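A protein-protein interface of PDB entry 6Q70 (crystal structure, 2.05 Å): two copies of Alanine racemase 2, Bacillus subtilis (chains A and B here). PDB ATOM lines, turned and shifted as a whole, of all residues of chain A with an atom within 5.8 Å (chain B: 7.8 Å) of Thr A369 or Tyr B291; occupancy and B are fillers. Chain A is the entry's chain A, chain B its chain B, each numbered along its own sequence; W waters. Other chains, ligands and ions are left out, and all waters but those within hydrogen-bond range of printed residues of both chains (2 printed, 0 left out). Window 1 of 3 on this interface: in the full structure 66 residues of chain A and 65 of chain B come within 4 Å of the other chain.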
ATOM      1  N   GLY A  44     -22.654  -4.751  12.083  1.00  0.00           N
ATOM      2  CA  GLY A  44     -22.443  -4.468  13.531  1.00  0.00           C
ATOM      3  C   GLY A  44     -23.046  -3.244  14.144  1.00  0.00           C
ATOM      4  O   GLY A  44     -22.773  -3.000  15.286  1.00  0.00           O
ATOM      5  N   ASP A 293     -14.836  -8.484  22.568  1.00  0.00           N
ATOM      6  CA  ASP A 293     -15.756  -7.489  22.066  1.00  0.00           C
ATOM      7  C   ASP A 293     -15.542  -7.160  20.533  1.00  0.00           C
ATOM      8  O   ASP A 293     -16.377  -6.549  19.871  1.00  0.00           O
ATOM      9  CB  ASP A 293     -15.548  -6.229  22.901  1.00  0.00           C
ATOM     10  CG  ASP A 293     -15.982  -6.412  24.346  1.00  0.00           C
ATOM     11  OD1 ASP A 293     -17.192  -6.721  24.625  1.00  0.00           O
ATOM     12  OD2 ASP A 293     -15.061  -6.285  25.220  1.00  0.00           O
ATOM     13  N   GLY A 294     -14.401  -7.539  20.015  1.00  0.00           N
ATOM     14  CA  GLY A 294     -13.952  -7.317  18.655  1.00  0.00           C
ATOM     15  C   GLY A 294     -12.857  -6.337  18.591  1.00  0.00           C
ATOM     16  O   GLY A 294     -12.547  -5.850  17.499  1.00  0.00           O
ATOM     17  N   ILE A 362      -9.943  -4.175   6.505  1.00  0.00           N
ATOM     18  CA  ILE A 362     -10.799  -3.132   5.868  1.00  0.00           C
ATOM     19  C   ILE A 362     -11.841  -2.825   6.917  1.00  0.00           C
ATOM     20  O   ILE A 362     -12.118  -3.724   7.799  1.00  0.00           O
ATOM     21  CB  ILE A 362     -11.502  -3.640   4.522  1.00  0.00           C
ATOM     22  CG1 ILE A 362     -12.227  -5.020   4.762  1.00  0.00           C
ATOM     23  CG2 ILE A 362     -10.470  -3.767   3.362  1.00  0.00           C
ATOM     24  CD1 ILE A 362     -12.892  -5.659   3.511  1.00  0.00           C
ATOM     25  N   TYR A 364     -15.073  -2.580   6.937  1.00  0.00           N
ATOM     26  CA  TYR A 364     -16.092  -3.630   7.011  1.00  0.00           C
ATOM     27  C   TYR A 364     -15.878  -4.630   8.100  1.00  0.00           C
ATOM     28  O   TYR A 364     -16.855  -4.946   8.825  1.00  0.00           O
ATOM     29  CB  TYR A 364     -16.152  -4.464   5.714  1.00  0.00           C
ATOM     30  CG  TYR A 364     -16.489  -3.753   4.387  1.00  0.00           C
ATOM     31  CD1 TYR A 364     -15.502  -3.158   3.603  1.00  0.00           C
ATOM     32  CD2 TYR A 364     -17.758  -3.860   3.834  1.00  0.00           C
ATOM     33  CE1 TYR A 364     -15.800  -2.561   2.360  1.00  0.00           C
ATOM     34  CE2 TYR A 364     -18.061  -3.325   2.591  1.00  0.00           C
ATOM     35  CZ  TYR A 364     -17.072  -2.677   1.874  1.00  0.00           C
ATOM     36  OH  TYR A 364     -17.442  -2.104   0.683  1.00  0.00           O
ATOM     37  N   GLU A 365     -14.656  -5.200   8.206  1.00  0.00           N
ATOM     38  CA  GLU A 365     -14.339  -6.206   9.233  1.00  0.00           C
ATOM     39  C   GLU A 365     -14.389  -5.513  10.597  1.00  0.00           C
ATOM     40  O   GLU A 365     -14.982  -6.089  11.571  1.00  0.00           O
ATOM     41  CB  GLU A 365     -12.964  -6.876   9.050  1.00  0.00           C
ATOM     42  CG  GLU A 365     -12.798  -8.056  10.000  1.00  0.00           C
ATOM     43  CD  GLU A 365     -11.624  -8.967   9.728  1.00  0.00           C
ATOM     44  OE1 GLU A 365     -10.630  -8.414   9.230  1.00  0.00           O
ATOM     45  OE2 GLU A 365     -11.710 -10.243  10.074  1.00  0.00           O
ATOM     46  N   VAL A 366     -13.792  -4.325  10.681  1.00  0.00           N
ATOM     47  CA  VAL A 366     -13.654  -3.652  11.949  1.00  0.00           C
ATOM     48  C   VAL A 366     -15.084  -3.456  12.558  1.00  0.00           C
ATOM     49  O   VAL A 366     -15.321  -3.766  13.739  1.00  0.00           O
ATOM     50  CB  VAL A 366     -12.948  -2.301  11.909  1.00  0.00           C
ATOM     51  CG1 VAL A 366     -13.043  -1.665  13.277  1.00  0.00           C
ATOM     52  CG2 VAL A 366     -11.455  -2.469  11.614  1.00  0.00           C
ATOM     53  N   VAL A 367     -16.050  -3.044  11.789  1.00  0.00           N
ATOM     54  CA  VAL A 367     -17.403  -2.824  12.430  1.00  0.00           C
ATOM     55  C   VAL A 367     -18.235  -4.042  12.507  1.00  0.00           C
ATOM     56  O   VAL A 367     -19.027  -4.175  13.457  1.00  0.00           O
ATOM     57  CB  VAL A 367     -18.221  -1.703  11.674  1.00  0.00           C
ATOM     58  CG1 VAL A 367     -17.666  -0.353  11.986  1.00  0.00           C
ATOM     59  CG2 VAL A 367     -18.208  -1.918  10.225  1.00  0.00           C
ATOM     60  N   SER A 368     -18.146  -4.952  11.498  1.00  0.00           N
ATOM     61  CA  SER A 368     -19.024  -6.081  11.459  1.00  0.00           C
ATOM     62  C   SER A 368     -18.569  -7.121  12.494  1.00  0.00           C
ATOM     63  O   SER A 368     -19.298  -8.106  12.654  1.00  0.00           O
ATOM     64  CB  SER A 368     -19.164  -6.767  10.070  1.00  0.00           C
ATOM     65  OG  SER A 368     -17.863  -7.193   9.571  1.00  0.00           O
ATOM     66  N   THR A 369     -17.408  -6.951  13.142  1.00  0.00           N
ATOM     67  CA  THR A 369     -17.061  -7.951  14.183  1.00  0.00           C
ATOM     68  C   THR A 369     -17.269  -7.404  15.614  1.00  0.00           C
ATOM     69  O   THR A 369     -16.774  -7.988  16.554  1.00  0.00           O
ATOM     70  CB  THR A 369     -15.588  -8.368  14.038  1.00  0.00           C
ATOM     71  OG1 THR A 369     -14.683  -7.238  14.069  1.00  0.00           O
ATOM     72  CG2 THR A 369     -15.397  -9.231  12.855  1.00  0.00           C
ATOM     73  N   LEU A 370     -17.956  -6.270  15.782  1.00  0.00           N
ATOM     74  CA  LEU A 370     -18.282  -5.740  17.104  1.00  0.00           C
ATOM     75  C   LEU A 370     -19.313  -6.647  17.770  1.00  0.00           C
ATOM     76  O   LEU A 370     -20.368  -6.896  17.226  1.00  0.00           O
ATOM     77  CB  LEU A 370     -18.810  -4.349  17.037  1.00  0.00           C
ATOM     78  CG  LEU A 370     -17.729  -3.379  16.690  1.00  0.00           C
ATOM     79  CD1 LEU A 370     -18.204  -2.008  16.320  1.00  0.00           C
ATOM     80  CD2 LEU A 370     -16.761  -3.317  17.895  1.00  0.00           C
ATOM     81  N   SER A 371     -18.938  -7.216  18.909  1.00  0.00           N
ATOM     82  CA  SER A 371     -19.747  -8.257  19.563  1.00  0.00           C
ATOM     83  C   SER A 371     -21.144  -7.755  19.946  1.00  0.00           C
ATOM     84  O   SER A 371     -21.335  -6.626  20.298  1.00  0.00           O
ATOM     85  CB  SER A 371     -19.078  -8.714  20.822  1.00  0.00           C
ATOM     86  OG  SER A 371     -19.861  -9.663  21.626  1.00  0.00           O
ATOM     87  N   ARG B   6     -29.123 -21.066   6.852  1.00  0.00           N
ATOM     88  CA  ARG B   6     -27.707 -20.882   6.566  1.00  0.00           C
ATOM     89  C   ARG B   6     -26.937 -21.905   7.324  1.00  0.00           C
ATOM     90  O   ARG B   6     -27.049 -21.983   8.556  1.00  0.00           O
ATOM     91  CB  ARG B   6     -27.274 -19.526   7.035  1.00  0.00           C
ATOM     92  CG  ARG B   6     -25.885 -19.169   6.550  1.00  0.00           C
ATOM     93  CD  ARG B   6     -25.446 -17.911   7.245  1.00  0.00           C
ATOM     94  NE  ARG B   6     -24.084 -17.559   6.923  1.00  0.00           N
ATOM     95  CZ  ARG B   6     -23.198 -17.029   7.766  1.00  0.00           C
ATOM     96  NH1 ARG B   6     -23.469 -16.817   9.053  1.00  0.00           N
ATOM     97  NH2 ARG B   6     -21.991 -16.673   7.302  1.00  0.00           N
ATOM     98  N   TYR B 272     -13.375 -10.879  -3.834  1.00  0.00           N
ATOM     99  CA  TYR B 272     -13.044  -9.459  -3.875  1.00  0.00           C
ATOM    100  C   TYR B 272     -11.566  -9.295  -4.183  1.00  0.00           C
ATOM    101  O   TYR B 272     -10.746 -10.074  -3.787  1.00  0.00           O
ATOM    102  CB  TYR B 272     -13.368  -8.817  -2.574  1.00  0.00           C
ATOM    103  CG  TYR B 272     -14.808  -8.542  -2.349  1.00  0.00           C
ATOM    104  CD1 TYR B 272     -15.474  -7.689  -3.184  1.00  0.00           C
ATOM    105  CD2 TYR B 272     -15.471  -9.047  -1.205  1.00  0.00           C
ATOM    106  CE1 TYR B 272     -16.802  -7.360  -2.973  1.00  0.00           C
ATOM    107  CE2 TYR B 272     -16.842  -8.745  -0.964  1.00  0.00           C
ATOM    108  CZ  TYR B 272     -17.475  -7.889  -1.869  1.00  0.00           C
ATOM    109  OH  TYR B 272     -18.773  -7.587  -1.753  1.00  0.00           O
ATOM    110  N   ILE B 289     -19.478 -19.192   5.600  1.00  0.00           N
ATOM    111  CA  ILE B 289     -18.840 -18.512   6.744  1.00  0.00           C
ATOM    112  C   ILE B 289     -17.933 -17.378   6.256  1.00  0.00           C
ATOM    113  O   ILE B 289     -17.381 -17.442   5.169  1.00  0.00           O
ATOM    114  CB  ILE B 289     -18.037 -19.474   7.620  1.00  0.00           C
ATOM    115  CG1 ILE B 289     -17.660 -18.801   8.911  1.00  0.00           C
ATOM    116  CG2 ILE B 289     -16.809 -19.997   6.889  1.00  0.00           C
ATOM    117  CD1 ILE B 289     -17.319 -19.771  10.026  1.00  0.00           C
ATOM    118  N   GLY B 290     -17.802 -16.335   7.055  1.00  0.00           N
ATOM    119  CA  GLY B 290     -17.028 -15.192   6.625  1.00  0.00           C
ATOM    120  C   GLY B 290     -16.535 -14.445   7.801  1.00  0.00           C
ATOM    121  O   GLY B 290     -16.723 -14.879   8.955  1.00  0.00           O
ATOM    122  N   TYR B 291     -15.955 -13.304   7.532  1.00  0.00           N
ATOM    123  CA  TYR B 291     -15.353 -12.493   8.602  1.00  0.00           C
ATOM    124  C   TYR B 291     -16.282 -11.915   9.629  1.00  0.00           C
ATOM    125  O   TYR B 291     -15.852 -11.638  10.736  1.00  0.00           O
ATOM    126  CB  TYR B 291     -14.317 -11.495   8.117  1.00  0.00           C
ATOM    127  CG  TYR B 291     -14.884 -10.413   7.177  1.00  0.00           C
ATOM    128  CD1 TYR B 291     -15.623  -9.363   7.705  1.00  0.00           C
ATOM    129  CD2 TYR B 291     -14.568 -10.392   5.865  1.00  0.00           C
ATOM    130  CE1 TYR B 291     -16.139  -8.387   6.867  1.00  0.00           C
ATOM    131  CE2 TYR B 291     -15.074  -9.354   4.942  1.00  0.00           C
ATOM    132  CZ  TYR B 291     -15.811  -8.372   5.475  1.00  0.00           C
ATOM    133  OH  TYR B 291     -16.275  -7.345   4.670  1.00  0.00           O
ATOM    134  N   ALA B 292     -17.549 -11.769   9.316  1.00  0.00           N
ATOM    135  CA  ALA B 292     -18.507 -11.256  10.392  1.00  0.00           C
ATOM    136  C   ALA B 292     -18.889 -12.364  11.335  1.00  0.00           C
ATOM    137  O   ALA B 292     -19.481 -12.068  12.400  1.00  0.00           O
ATOM    138  CB  ALA B 292     -19.748 -10.599   9.840  1.00  0.00           C
ATOM    139  N   ASP B 293     -18.685 -13.627  10.918  1.00  0.00           N
ATOM    140  CA  ASP B 293     -18.783 -14.780  11.864  1.00  0.00           C
ATOM    141  C   ASP B 293     -17.581 -14.905  12.831  1.00  0.00           C
ATOM    142  O   ASP B 293     -17.632 -15.728  13.735  1.00  0.00           O
ATOM    143  CB  ASP B 293     -19.000 -16.117  11.140  1.00  0.00           C
ATOM    144  CG  ASP B 293     -20.151 -16.073  10.211  1.00  0.00           C
ATOM    145  OD1 ASP B 293     -21.314 -16.166  10.714  1.00  0.00           O
ATOM    146  OD2 ASP B 293     -19.855 -15.848   8.995  1.00  0.00           O
ATOM    147  N   GLY B 294     -16.453 -14.203  12.578  1.00  0.00           N
ATOM    148  CA  GLY B 294     -15.187 -14.366  13.348  1.00  0.00           C
ATOM    149  C   GLY B 294     -14.122 -15.186  12.650  1.00  0.00           C
ATOM    150  O   GLY B 294     -13.137 -15.536  13.233  1.00  0.00           O
ATOM    151  N   TYR B 295     -14.323 -15.475  11.355  1.00  0.00           N
ATOM    152  CA  TYR B 295     -13.377 -16.246  10.513  1.00  0.00           C
ATOM    153  C   TYR B 295     -12.498 -15.198   9.855  1.00  0.00           C
ATOM    154  O   TYR B 295     -12.995 -14.496   8.885  1.00  0.00           O
ATOM    155  CB  TYR B 295     -14.151 -17.092   9.402  1.00  0.00           C
ATOM    156  CG  TYR B 295     -13.213 -18.022   8.758  1.00  0.00           C
ATOM    157  CD1 TYR B 295     -12.799 -19.145   9.426  1.00  0.00           C
ATOM    158  CD2 TYR B 295     -12.726 -17.803   7.484  1.00  0.00           C
ATOM    159  CE1 TYR B 295     -11.913 -20.056   8.842  1.00  0.00           C
ATOM    160  CE2 TYR B 295     -11.848 -18.684   6.903  1.00  0.00           C
ATOM    161  CZ  TYR B 295     -11.473 -19.849   7.617  1.00  0.00           C
ATOM    162  OH  TYR B 295     -10.582 -20.766   7.094  1.00  0.00           O
ATOM    163  N   SER B 296     -11.294 -14.977  10.421  1.00  0.00           N
ATOM    164  CA  SER B 296     -10.460 -13.766  10.019  1.00  0.00           C
ATOM    165  C   SER B 296     -10.285 -13.585   8.550  1.00  0.00           C
ATOM    166  O   SER B 296      -9.990 -14.551   7.824  1.00  0.00           O
ATOM    167  CB  SER B 296      -9.032 -13.780  10.619  1.00  0.00           C
ATOM    168  OG  SER B 296      -8.369 -12.536  10.569  1.00  0.00           O
ATOM    169  N   ARG B 297     -10.421 -12.329   8.140  1.00  0.00           N
ATOM    170  CA  ARG B 297     -10.152 -11.934   6.803  1.00  0.00           C
ATOM    171  C   ARG B 297      -8.636 -12.118   6.479  1.00  0.00           C
ATOM    172  O   ARG B 297      -8.295 -12.171   5.319  1.00  0.00           O
ATOM    173  CB  ARG B 297     -10.535 -10.514   6.592  1.00  0.00           C
ATOM    174  CG  ARG B 297     -10.407 -10.055   5.119  1.00  0.00           C
ATOM    175  CD  ARG B 297     -11.020  -8.712   4.890  1.00  0.00           C
ATOM    176  NE  ARG B 297     -10.675  -8.211   3.565  1.00  0.00           N
ATOM    177  CZ  ARG B 297      -9.581  -7.567   3.162  1.00  0.00           C
ATOM    178  NH1 ARG B 297      -9.554  -7.192   1.912  1.00  0.00           N
ATOM    179  NH2 ARG B 297      -8.518  -7.315   3.928  1.00  0.00           N
ATOM    180  N   ALA B 298      -7.754 -12.148   7.505  1.00  0.00           N
ATOM    181  CA  ALA B 298      -6.355 -12.415   7.304  1.00  0.00           C
ATOM    182  C   ALA B 298      -6.160 -13.846   6.828  1.00  0.00           C
ATOM    183  O   ALA B 298      -5.100 -14.173   6.296  1.00  0.00           O
ATOM    184  CB  ALA B 298      -5.481 -12.002   8.487  1.00  0.00           C
ATOM    185  N   SER B 300      -7.565 -14.922   4.120  1.00  0.00           N
ATOM    186  CA  SER B 300      -7.635 -14.723   2.679  1.00  0.00           C
ATOM    187  C   SER B 300      -6.363 -15.283   2.020  1.00  0.00           C
ATOM    188  O   SER B 300      -5.274 -15.015   2.524  1.00  0.00           O
ATOM    189  CB  SER B 300      -7.786 -13.243   2.339  1.00  0.00           C
ATOM    190  OG  SER B 300      -9.077 -12.690   2.742  1.00  0.00           O
ATOM    191  N   ARG B 317     -10.234 -13.786  -1.444  1.00  0.00           N
ATOM    192  CA  ARG B 317     -10.514 -13.201  -0.175  1.00  0.00           C
ATOM    193  C   ARG B 317     -11.688 -13.802   0.590  1.00  0.00           C
ATOM    194  O   ARG B 317     -12.673 -14.209  -0.006  1.00  0.00           O
ATOM    195  CB  ARG B 317     -10.732 -11.745  -0.369  1.00  0.00           C
ATOM    196  CG  ARG B 317      -9.443 -11.072  -0.721  1.00  0.00           C
ATOM    197  CD  ARG B 317      -9.567  -9.642  -0.320  1.00  0.00           C
ATOM    198  NE  ARG B 317      -8.619  -8.821  -1.083  1.00  0.00           N
ATOM    199  CZ  ARG B 317      -8.858  -7.693  -1.752  1.00  0.00           C
ATOM    200  NH1 ARG B 317     -10.056  -7.052  -1.790  1.00  0.00           N
ATOM    201  NH2 ARG B 317      -7.826  -7.151  -2.403  1.00  0.00           N
ATOM    202  N   VAL B 318     -11.555 -13.833   1.921  1.00  0.00           N
ATOM    203  CA  VAL B 318     -12.700 -14.043   2.855  1.00  0.00           C
ATOM    204  C   VAL B 318     -13.633 -12.846   2.640  1.00  0.00           C
ATOM    205  O   VAL B 318     -13.167 -11.797   2.575  1.00  0.00           O
ATOM    206  CB  VAL B 318     -12.226 -14.131   4.359  1.00  0.00           C
ATOM    207  CG1 VAL B 318     -13.409 -14.267   5.275  1.00  0.00           C
ATOM    208  CG2 VAL B 318     -11.196 -15.239   4.590  1.00  0.00           C
ATOM    209  N   THR B 319     -14.934 -13.046   2.534  1.00  0.00           N
ATOM    210  CA  THR B 319     -15.964 -11.970   2.444  1.00  0.00           C
ATOM    211  C   THR B 319     -16.713 -11.977   3.740  1.00  0.00           C
ATOM    212  O   THR B 319     -16.387 -12.787   4.673  1.00  0.00           O
ATOM    213  CB  THR B 319     -16.897 -12.183   1.199  1.00  0.00           C
ATOM    214  OG1 THR B 319     -17.751 -13.342   1.302  1.00  0.00           O
ATOM    215  CG2 THR B 319     -15.960 -12.512  -0.043  1.00  0.00           C
ATOM    216  N   MET B 320     -17.691 -11.103   3.838  1.00  0.00           N
ATOM    217  CA  MET B 320     -18.316 -10.828   5.099  1.00  0.00           C
ATOM    218  C   MET B 320     -19.059 -12.064   5.589  1.00  0.00           C
ATOM    219  O   MET B 320     -19.006 -12.359   6.755  1.00  0.00           O
ATOM    220  CB  MET B 320     -19.244  -9.611   4.992  1.00  0.00           C
ATOM    221  CG  MET B 320     -19.862  -9.321   6.369  1.00  0.00           C
ATOM    222  SD  MET B 320     -20.820  -7.830   6.416  1.00  0.00           S
ATOM    223  CE  MET B 320     -19.501  -6.616   6.255  1.00  0.00           C
ATOM    224  N   ASP B 321     -19.678 -12.822   4.669  1.00  0.00           N
ATOM    225  CA  ASP B 321     -20.519 -13.965   5.004  1.00  0.00           C
ATOM    226  C   ASP B 321     -20.131 -15.286   4.366  1.00  0.00           C
ATOM    227  O   ASP B 321     -20.727 -16.304   4.727  1.00  0.00           O
ATOM    228  CB  ASP B 321     -22.005 -13.654   4.658  1.00  0.00           C
ATOM    229  CG  ASP B 321     -22.443 -12.291   5.165  1.00  0.00           C
ATOM    230  OD1 ASP B 321     -22.224 -12.031   6.403  1.00  0.00           O
ATOM    231  OD2 ASP B 321     -22.921 -11.525   4.292  1.00  0.00           O
ATOM    232  N   MET B 322     -19.119 -15.318   3.491  1.00  0.00           N
ATOM    233  CA  MET B 322     -18.784 -16.499   2.724  1.00  0.00           C
ATOM    234  C   MET B 322     -17.277 -16.531   2.389  1.00  0.00           C
ATOM    235  O   MET B 322     -16.575 -15.462   2.404  1.00  0.00           O
ATOM    236  CB  MET B 322     -19.570 -16.550   1.421  1.00  0.00           C
ATOM    237  CG  MET B 322     -21.034 -17.053   1.424  1.00  0.00           C
ATOM    238  SD  MET B 322     -21.946 -16.715  -0.164  1.00  0.00           S
ATOM    239  CE  MET B 322     -22.581 -15.056   0.018  1.00  0.00           C
ATOM    240  N   ILE B 323     -16.822 -17.754   2.149  1.00  0.00           N
ATOM    241  CA  ILE B 323     -15.555 -18.028   1.575  1.00  0.00           C
ATOM    242  C   ILE B 323     -15.672 -19.023   0.493  1.00  0.00           C
ATOM    243  O   ILE B 323     -16.617 -19.799   0.445  1.00  0.00           O
ATOM    244  CB  ILE B 323     -14.549 -18.543   2.657  1.00  0.00           C
ATOM    245  CG1 ILE B 323     -15.042 -19.799   3.333  1.00  0.00           C
ATOM    246  CG2 ILE B 323     -14.315 -17.460   3.693  1.00  0.00           C
ATOM    247  CD1 ILE B 323     -14.038 -20.494   4.199  1.00  0.00           C
ATOM    248  N   THR B 369     -14.189 -14.867  19.691  1.00  0.00           N
ATOM    249  CA  THR B 369     -14.765 -13.957  18.715  1.00  0.00           C
ATOM    250  C   THR B 369     -15.725 -14.654  17.769  1.00  0.00           C
ATOM    251  O   THR B 369     -16.127 -14.112  16.722  1.00  0.00           O
ATOM    252  CB  THR B 369     -13.613 -13.251  17.921  1.00  0.00           C
ATOM    253  OG1 THR B 369     -12.736 -14.256  17.486  1.00  0.00           O
ATOM    254  CG2 THR B 369     -12.783 -12.384  18.877  1.00  0.00           C
ATOM    255  N   SER B 371     -19.017 -15.434  16.354  1.00  0.00           N
ATOM    256  CA  SER B 371     -20.250 -14.607  16.427  1.00  0.00           C
ATOM    257  C   SER B 371     -21.470 -15.350  16.950  1.00  0.00           C
ATOM    258  O   SER B 371     -21.619 -16.580  16.704  1.00  0.00           O
ATOM    259  CB  SER B 371     -20.572 -14.041  15.061  1.00  0.00           C
ATOM    260  OG  SER B 371     -21.843 -13.447  15.032  1.00  0.00           O
ATOM    261  N   ARG B 373     -24.239 -15.199  15.801  1.00  0.00           N
ATOM    262  CA  ARG B 373     -25.119 -15.659  14.711  1.00  0.00           C
ATOM    263  C   ARG B 373     -24.910 -17.144  14.254  1.00  0.00           C
ATOM    264  O   ARG B 373     -25.697 -17.673  13.509  1.00  0.00           O
ATOM    265  CB  ARG B 373     -25.064 -14.620  13.598  1.00  0.00           C
ATOM    266  CG  ARG B 373     -23.986 -14.736  12.605  1.00  0.00           C
ATOM    267  CD  ARG B 373     -24.349 -13.897  11.317  1.00  0.00           C
ATOM    268  NE  ARG B 373     -23.109 -13.925  10.446  1.00  0.00           N
ATOM    269  CZ  ARG B 373     -22.900 -13.251   9.346  1.00  0.00           C
ATOM    270  NH1 ARG B 373     -23.801 -12.405   8.886  1.00  0.00           N
ATOM    271  NH2 ARG B 373     -21.730 -13.384   8.717  1.00  0.00           N
HETATM  272  O   HOH W   1      -8.218  -9.623   8.906  1.00  0.00           O
HETATM  273  O   HOH W   2     -13.219 -11.691  11.642  1.00  0.00           O
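Ile A362 touches Tyr B291. Ile A362 touches Arg B297. Tyr A364 touches Tyr B291. OE2 of Glu A365 touches CB of Tyr B291 (3.5 Å). CA of Ser B296 touches OE2 of Glu A365, 3.7 Å away. Ser A368 touches Tyr B291 (OG to CE1, 3.4 Å). Ser A368 touches Ala B292. CE of Met B320 touches OG of Ser A368, 3.7 Å away. Thr A369 touches Tyr B291 (CG2 to O, 3.2 Å).
Positions printed for both chains: 293, 294, 369 and 371. Of the 10 pairs that touch across the chains among the printed residues, none has its exchanged pair printed and touching as well.
The side-chain hydroxyl of Ser A368 sits at hydrogen-bond distance from the backbone carbonyl oxygen of Tyr A364. The side-chain hydroxyl (OG) of Ser B296 lies close to the backbone NH (N) of Ala B298 (3.1 Å). N of Ala B292 lies within hydrogen-bond range of O of Met B320 (3.0 Å). O of Arg B297 sits at hydrogen-bond distance from OG of Ser B300 (2.7 Å). The backbone carbonyl oxygen (O) of Thr B319 is in hydrogen-bond range of the backbone NH (N) of Tyr B291 (2.9 Å). The backbone carbonyl oxygen of Met B320 is in hydrogen-bond range of the backbone NH of Tyr B291 (3.3 Å).
Tyr B291 touches just these residues of chain A: Ile A362 (3.95 Å), Tyr A364 (3.1 Å), Glu A365 (3.5 Å), Ser A368 (3.4 Å) and Thr A369 (3.2 Å). Of the printed residues of chain A, Ala B292 touches Ser A368. Printed residues of chain B within 4 Å of Glu A365: Tyr B291, Ser B296 and Arg B297. Printed residues of chain B within 4 Å of Tyr A364: Tyr B291. Printed residues of chain A within 4 Å of Ser B296: Glu A365. Asp A293 touches none of the printed residues of chain B. The nearest printed residue of chain A that does not touch Tyr B291 is Val A366 (6.0 Å). The nearest printed residue of chain A that does not touch Ser B296 is Thr A369 (7.3 Å).
Printed residues of chain B that touch a printed residue of chain A: Tyr B291, Ala B292, Ser B296, Arg B297 and Met B320. Hydrophobic or aromatic side chains of chain A that line the printed part of chain B: Ile A362 and Tyr A364.
Water W2 bridges the side-chain carboxylate (OE2) of Glu A365 (2.6 Å) and the backbone carbonyl oxygen (O) of Tyr B291 (2.8 Å). Water W1 lies within hydrogen-bond range of OE1 of Glu A365 (2.7 Å), N of Ala B298 (2.9 Å) and OG of Ser B296 (3.4 Å).
N of Arg B297 sits at hydrogen-bond distance from OE2 of Glu A365, at 3.1 Å.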
